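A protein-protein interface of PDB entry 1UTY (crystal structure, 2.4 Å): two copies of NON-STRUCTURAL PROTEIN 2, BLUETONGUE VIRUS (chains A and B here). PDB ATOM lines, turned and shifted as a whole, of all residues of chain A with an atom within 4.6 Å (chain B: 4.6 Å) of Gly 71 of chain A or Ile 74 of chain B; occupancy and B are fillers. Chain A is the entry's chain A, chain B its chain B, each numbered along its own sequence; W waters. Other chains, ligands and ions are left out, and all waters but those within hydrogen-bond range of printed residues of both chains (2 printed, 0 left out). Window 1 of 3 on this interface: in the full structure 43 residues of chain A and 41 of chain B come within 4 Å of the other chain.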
ATOM      1  N   GLN A  69     -21.261  -1.092  -0.179  1.00  0.00           N
ATOM      2  CA  GLN A  69     -20.206  -0.217  -0.691  1.00  0.00           C
ATOM      3  C   GLN A  69     -19.646  -0.605  -2.052  1.00  0.00           C
ATOM      4  O   GLN A  69     -18.839  -1.537  -2.208  1.00  0.00           O
ATOM      5  CB  GLN A  69     -19.109   0.004   0.340  1.00  0.00           C
ATOM      6  CG  GLN A  69     -19.149   1.409   0.887  1.00  0.00           C
ATOM      7  CD  GLN A  69     -19.273   1.439   2.382  1.00  0.00           C
ATOM      8  OE1 GLN A  69     -19.593   0.425   2.997  1.00  0.00           O
ATOM      9  NE2 GLN A  69     -19.005   2.599   2.983  1.00  0.00           N
ATOM     10  N   ASP A  70     -20.094   0.159  -3.032  1.00  0.00           N
ATOM     11  CA  ASP A  70     -19.816  -0.115  -4.416  1.00  0.00           C
ATOM     12  C   ASP A  70     -19.103   1.090  -5.022  1.00  0.00           C
ATOM     13  O   ASP A  70     -19.638   1.782  -5.892  1.00  0.00           O
ATOM     14  CB  ASP A  70     -21.132  -0.420  -5.135  1.00  0.00           C
ATOM     15  CG  ASP A  70     -20.922  -0.932  -6.527  1.00  0.00           C
ATOM     16  OD1 ASP A  70     -19.746  -1.201  -6.889  1.00  0.00           O
ATOM     17  OD2 ASP A  70     -21.878  -1.080  -7.331  1.00  0.00           O
ATOM     18  N   GLY A  71     -17.882   1.330  -4.552  1.00  0.00           N
ATOM     19  CA  GLY A  71     -17.106   2.466  -5.013  1.00  0.00           C
ATOM     20  C   GLY A  71     -17.719   3.765  -4.550  1.00  0.00           C
ATOM     21  O   GLY A  71     -17.802   4.023  -3.341  1.00  0.00           O
ATOM     22  N   GLN A  72     -18.172   4.565  -5.512  1.00  0.00           N
ATOM     23  CA  GLN A  72     -18.813   5.845  -5.220  1.00  0.00           C
ATOM     24  C   GLN A  72     -20.282   5.658  -4.820  1.00  0.00           C
ATOM     25  O   GLN A  72     -20.844   6.497  -4.122  1.00  0.00           O
ATOM     26  CB  GLN A  72     -18.697   6.794  -6.425  1.00  0.00           C
ATOM     27  N   ASP A  73     -20.889   4.553  -5.264  1.00  0.00           N
ATOM     28  CA  ASP A  73     -22.274   4.219  -4.943  1.00  0.00           C
ATOM     29  C   ASP A  73     -22.355   3.541  -3.582  1.00  0.00           C
ATOM     30  O   ASP A  73     -21.846   2.432  -3.393  1.00  0.00           O
ATOM     31  CB  ASP A  73     -22.875   3.303  -6.010  1.00  0.00           C
ATOM     32  CG  ASP A  73     -23.058   3.992  -7.345  1.00  0.00           C
ATOM     33  OD1 ASP A  73     -23.083   5.242  -7.401  1.00  0.00           O
ATOM     34  OD2 ASP A  73     -23.184   3.356  -8.409  1.00  0.00           O
ATOM     35  N   ILE A  74     -22.992   4.225  -2.637  1.00  0.00           N
ATOM     36  CA  ILE A  74     -23.161   3.726  -1.273  1.00  0.00           C
ATOM     37  C   ILE A  74     -24.651   3.702  -0.931  1.00  0.00           C
ATOM     38  O   ILE A  74     -25.321   4.741  -0.972  1.00  0.00           O
ATOM     39  CB  ILE A  74     -22.368   4.609  -0.273  1.00  0.00           C
ATOM     40  CG1 ILE A  74     -20.890   4.697  -0.682  1.00  0.00           C
ATOM     41  CG2 ILE A  74     -22.434   4.036   1.098  1.00  0.00           C
ATOM     42  CD1 ILE A  74     -20.183   5.952  -0.245  1.00  0.00           C
ATOM     43  N   ARG B  67     -10.518  -1.764   4.244  1.00  0.00           N
ATOM     44  CA  ARG B  67     -11.011  -0.620   3.515  1.00  0.00           C
ATOM     45  C   ARG B  67     -11.689   0.341   4.470  1.00  0.00           C
ATOM     46  O   ARG B  67     -12.697   0.002   5.066  1.00  0.00           O
ATOM     47  CB  ARG B  67     -12.024  -1.054   2.470  1.00  0.00           C
ATOM     48  CG  ARG B  67     -11.806  -0.381   1.171  1.00  0.00           C
ATOM     49  CD  ARG B  67     -13.027   0.052   0.445  1.00  0.00           C
ATOM     50  NE  ARG B  67     -13.478  -0.903  -0.562  1.00  0.00           N
ATOM     51  CZ  ARG B  67     -12.804  -1.300  -1.660  1.00  0.00           C
ATOM     52  NH1 ARG B  67     -11.571  -0.859  -1.950  1.00  0.00           N
ATOM     53  NH2 ARG B  67     -13.385  -2.170  -2.481  1.00  0.00           N
ATOM     54  N   ILE B  68     -11.118   1.530   4.625  1.00  0.00           N
ATOM     55  CA  ILE B  68     -11.765   2.570   5.398  1.00  0.00           C
ATOM     56  C   ILE B  68     -12.700   3.279   4.445  1.00  0.00           C
ATOM     57  O   ILE B  68     -12.267   3.802   3.434  1.00  0.00           O
ATOM     58  CB  ILE B  68     -10.730   3.555   6.008  1.00  0.00           C
ATOM     59  CG1 ILE B  68      -9.798   2.842   6.999  1.00  0.00           C
ATOM     60  CG2 ILE B  68     -11.438   4.730   6.659  1.00  0.00           C
ATOM     61  CD1 ILE B  68      -8.400   3.512   7.158  1.00  0.00           C
ATOM     62  N   GLY B  71     -17.345   7.905   3.709  1.00  0.00           N
ATOM     63  CA  GLY B  71     -18.139   8.593   2.707  1.00  0.00           C
ATOM     64  C   GLY B  71     -17.554   8.313   1.340  1.00  0.00           C
ATOM     65  O   GLY B  71     -17.484   7.153   0.920  1.00  0.00           O
ATOM     66  N   GLN B  72     -17.123   9.368   0.652  1.00  0.00           N
ATOM     67  CA  GLN B  72     -16.458   9.224  -0.645  1.00  0.00           C
ATOM     68  C   GLN B  72     -14.936   9.094  -0.485  1.00  0.00           C
ATOM     69  O   GLN B  72     -14.226   8.794  -1.451  1.00  0.00           O
ATOM     70  CB  GLN B  72     -16.812  10.388  -1.576  1.00  0.00           C
ATOM     71  CG  GLN B  72     -18.279  10.425  -2.036  1.00  0.00           C
ATOM     72  CD  GLN B  72     -18.599   9.406  -3.124  1.00  0.00           C
ATOM     73  OE1 GLN B  72     -17.697   8.768  -3.681  1.00  0.00           O
ATOM     74  NE2 GLN B  72     -19.889   9.245  -3.425  1.00  0.00           N
ATOM     75  N   ASP B  73     -14.443   9.345   0.730  1.00  0.00           N
ATOM     76  CA  ASP B  73     -13.072   9.012   1.099  1.00  0.00           C
ATOM     77  C   ASP B  73     -12.945   7.513   1.332  1.00  0.00           C
ATOM     78  O   ASP B  73     -13.366   6.992   2.368  1.00  0.00           O
ATOM     79  CB  ASP B  73     -12.667   9.747   2.369  1.00  0.00           C
ATOM     80  CG  ASP B  73     -12.204  11.151   2.102  1.00  0.00           C
ATOM     81  OD1 ASP B  73     -12.772  11.823   1.224  1.00  0.00           O
ATOM     82  OD2 ASP B  73     -11.274  11.674   2.740  1.00  0.00           O
ATOM     83  N   ILE B  74     -12.368   6.817   0.361  1.00  0.00           N
ATOM     84  CA  ILE B  74     -12.160   5.386   0.474  1.00  0.00           C
ATOM     85  C   ILE B  74     -10.666   5.052   0.443  1.00  0.00           C
ATOM     86  O   ILE B  74      -9.970   5.292  -0.551  1.00  0.00           O
ATOM     87  CB  ILE B  74     -12.955   4.639  -0.636  1.00  0.00           C
ATOM     88  CG1 ILE B  74     -14.391   5.161  -0.707  1.00  0.00           C
ATOM     89  CG2 ILE B  74     -13.012   3.164  -0.345  1.00  0.00           C
ATOM     90  CD1 ILE B  74     -15.125   4.749  -1.937  1.00  0.00           C
ATOM     91  N   ILE B  75     -10.177   4.501   1.543  1.00  0.00           N
ATOM     92  CA  ILE B  75      -8.774   4.110   1.641  1.00  0.00           C
ATOM     93  C   ILE B  75      -8.684   2.602   1.776  1.00  0.00           C
ATOM     94  O   ILE B  75      -9.232   2.029   2.723  1.00  0.00           O
ATOM     95  CB  ILE B  75      -8.076   4.783   2.853  1.00  0.00           C
ATOM     96  CG1 ILE B  75      -8.272   6.305   2.819  1.00  0.00           C
ATOM     97  CG2 ILE B  75      -6.592   4.444   2.857  1.00  0.00           C
ATOM     98  CD1 ILE B  75      -8.760   6.861   4.106  1.00  0.00           C
ATOM     99  N   SER B  76      -7.966   1.987   0.843  1.00  0.00           N
ATOM    100  CA  SER B  76      -7.848   0.539   0.779  1.00  0.00           C
ATOM    101  C   SER B  76      -6.416   0.100   1.064  1.00  0.00           C
ATOM    102  O   SER B  76      -5.471   0.564   0.404  1.00  0.00           O
ATOM    103  CB  SER B  76      -8.308   0.044  -0.594  1.00  0.00           C
ATOM    104  OG  SER B  76      -9.545   0.648  -0.942  1.00  0.00           O
ATOM    105  N   THR B  87      -3.916   2.748  -1.021  1.00  0.00           N
ATOM    106  CA  THR B  87      -4.391   3.594  -2.090  1.00  0.00           C
ATOM    107  C   THR B  87      -5.686   4.252  -1.663  1.00  0.00           C
ATOM    108  O   THR B  87      -6.422   3.745  -0.818  1.00  0.00           O
ATOM    109  CB  THR B  87      -4.556   2.794  -3.428  1.00  0.00           C
ATOM    110  OG1 THR B  87      -4.951   3.681  -4.487  1.00  0.00           O
ATOM    111  CG2 THR B  87      -5.699   1.778  -3.343  1.00  0.00           C
ATOM    112  N   THR B  88      -5.940   5.389  -2.277  1.00  0.00           N
ATOM    113  CA  THR B  88      -7.060   6.257  -1.973  1.00  0.00           C
ATOM    114  C   THR B  88      -7.994   6.143  -3.177  1.00  0.00           C
ATOM    115  O   THR B  88      -9.074   6.730  -3.218  1.00  0.00           O
ATOM    116  CB  THR B  88      -6.487   7.671  -1.809  1.00  0.00           C
ATOM    117  OG1 THR B  88      -6.546   8.045  -0.430  1.00  0.00           O
ATOM    118  CG2 THR B  88      -7.296   8.700  -2.507  1.00  0.00           C
ATOM    119  N   GLU B  89      -7.544   5.369  -4.157  1.00  0.00           N
ATOM    120  CA  GLU B  89      -8.258   5.165  -5.395  1.00  0.00           C
ATOM    121  C   GLU B  89      -8.880   3.784  -5.396  1.00  0.00           C
ATOM    122  O   GLU B  89      -8.583   2.943  -4.535  1.00  0.00           O
ATOM    123  CB  GLU B  89      -7.301   5.287  -6.569  1.00  0.00           C
ATOM    124  CG  GLU B  89      -7.750   6.306  -7.604  1.00  0.00           C
ATOM    125  CD  GLU B  89      -6.983   7.600  -7.509  1.00  0.00           C
ATOM    126  OE1 GLU B  89      -6.587   7.982  -6.388  1.00  0.00           O
ATOM    127  OE2 GLU B  89      -6.771   8.235  -8.558  1.00  0.00           O
ATOM    128  N   ARG B  90      -9.750   3.554  -6.366  1.00  0.00           N
ATOM    129  CA  ARG B  90     -10.483   2.314  -6.470  1.00  0.00           C
ATOM    130  C   ARG B  90      -9.514   1.149  -6.608  1.00  0.00           C
ATOM    131  O   ARG B  90      -8.455   1.269  -7.227  1.00  0.00           O
ATOM    132  CB  ARG B  90     -11.430   2.381  -7.672  1.00  0.00           C
ATOM    133  CG  ARG B  90     -12.666   1.540  -7.507  1.00  0.00           C
ATOM    134  CD  ARG B  90     -13.896   2.086  -8.204  1.00  0.00           C
ATOM    135  NE  ARG B  90     -15.002   1.120  -8.265  1.00  0.00           N
ATOM    136  CZ  ARG B  90     -15.482   0.432  -7.229  1.00  0.00           C
ATOM    137  NH1 ARG B  90     -14.952   0.567  -6.013  1.00  0.00           N
ATOM    138  NH2 ARG B  90     -16.500  -0.404  -7.413  1.00  0.00           N
HETATM  139  O   HOH W   1     -19.163   5.105   3.624  1.00  0.00           O
HETATM  140  O   HOH W   2     -16.018   1.015  -1.784  1.00  0.00           O
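Hydrophobic or aromatic side chains of chain B within 4 Å of the printed part of chain A: Ile 74. Of the 6 printed residues of chain A, 4 touch a printed residue of chain B. Along chain A the printed residues that touch a printed residue of chain B span positions 70 to 74. Among the printed residues, 5 pairs touch across the chains.
Gly 71 of chain A touches Ile 74 of chain B, and with the chains exchanged Ile 74 of chain A touches Gly 71 of chain B. Gln 72 of chain A touches its own counterpart, Gln 72 of chain B. Positions printed for both chains: 71, 72, 73 and 74. Of the 5 pairs that touch across the chains among the printed residues, 3 have their exchanged pair printed and touching as well.
The backbone NH (N) of Gly 71 of chain A lies close to the guanidinium group (NH1) of Arg 90 of chain B. The backbone carbonyl oxygen of Gln 72 of chain A lies within hydrogen-bond range of the side-chain amide nitrogen of Gln 72 of chain B (3.0 Å). The side-chain carboxylate of Asp 70 of chain A is in salt-bridge range of the guanidinium group of Arg 90 of chain B (3.4 Å).
Among the printed residues, merely in contact across the chains: Gly 71 of chain A with Ile 74 of chain B (3.1 Å) and Ile 74 of chain A with Gly 71 of chain B (3.2 Å).
Water W1 lies within hydrogen-bond range of the side-chain amide nitrogen (NE2) of Gln 69 of chain A and the backbone NH (N) of Gly 71 of chain B. Water W2 bridges N of Gly 71 of chain A (3.4 Å) and NE of Arg 67 of chain B (3.4 Å).
Gly 71 of chain A touches just these residues of chain B: Ile 74 and Arg 90. Of the printed residues of chain A, Ile 74 of chain B touches Gly 71. Printed residues of chain A within 4 Å of Arg 90 of chain B: Asp 70 (3.4 Å) and Gly 71 (3.0 Å). Printed residues of chain A within 4 Å of Gly 71 of chain B: Ile 74. Of the printed residues of chain A, Gln 72 of chain B touches Gln 72. Of the printed residues of chain B, Ile 74 of chain A touches Gly 71. The nearest printed residue of chain B that does not touch Gly 71 of chain A is Gln 72 of chain B (4.8 Å). The nearest printed residue of chain B that does not touch Gln 72 of chain A is Ile 74 of chain B (4.7 Å).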
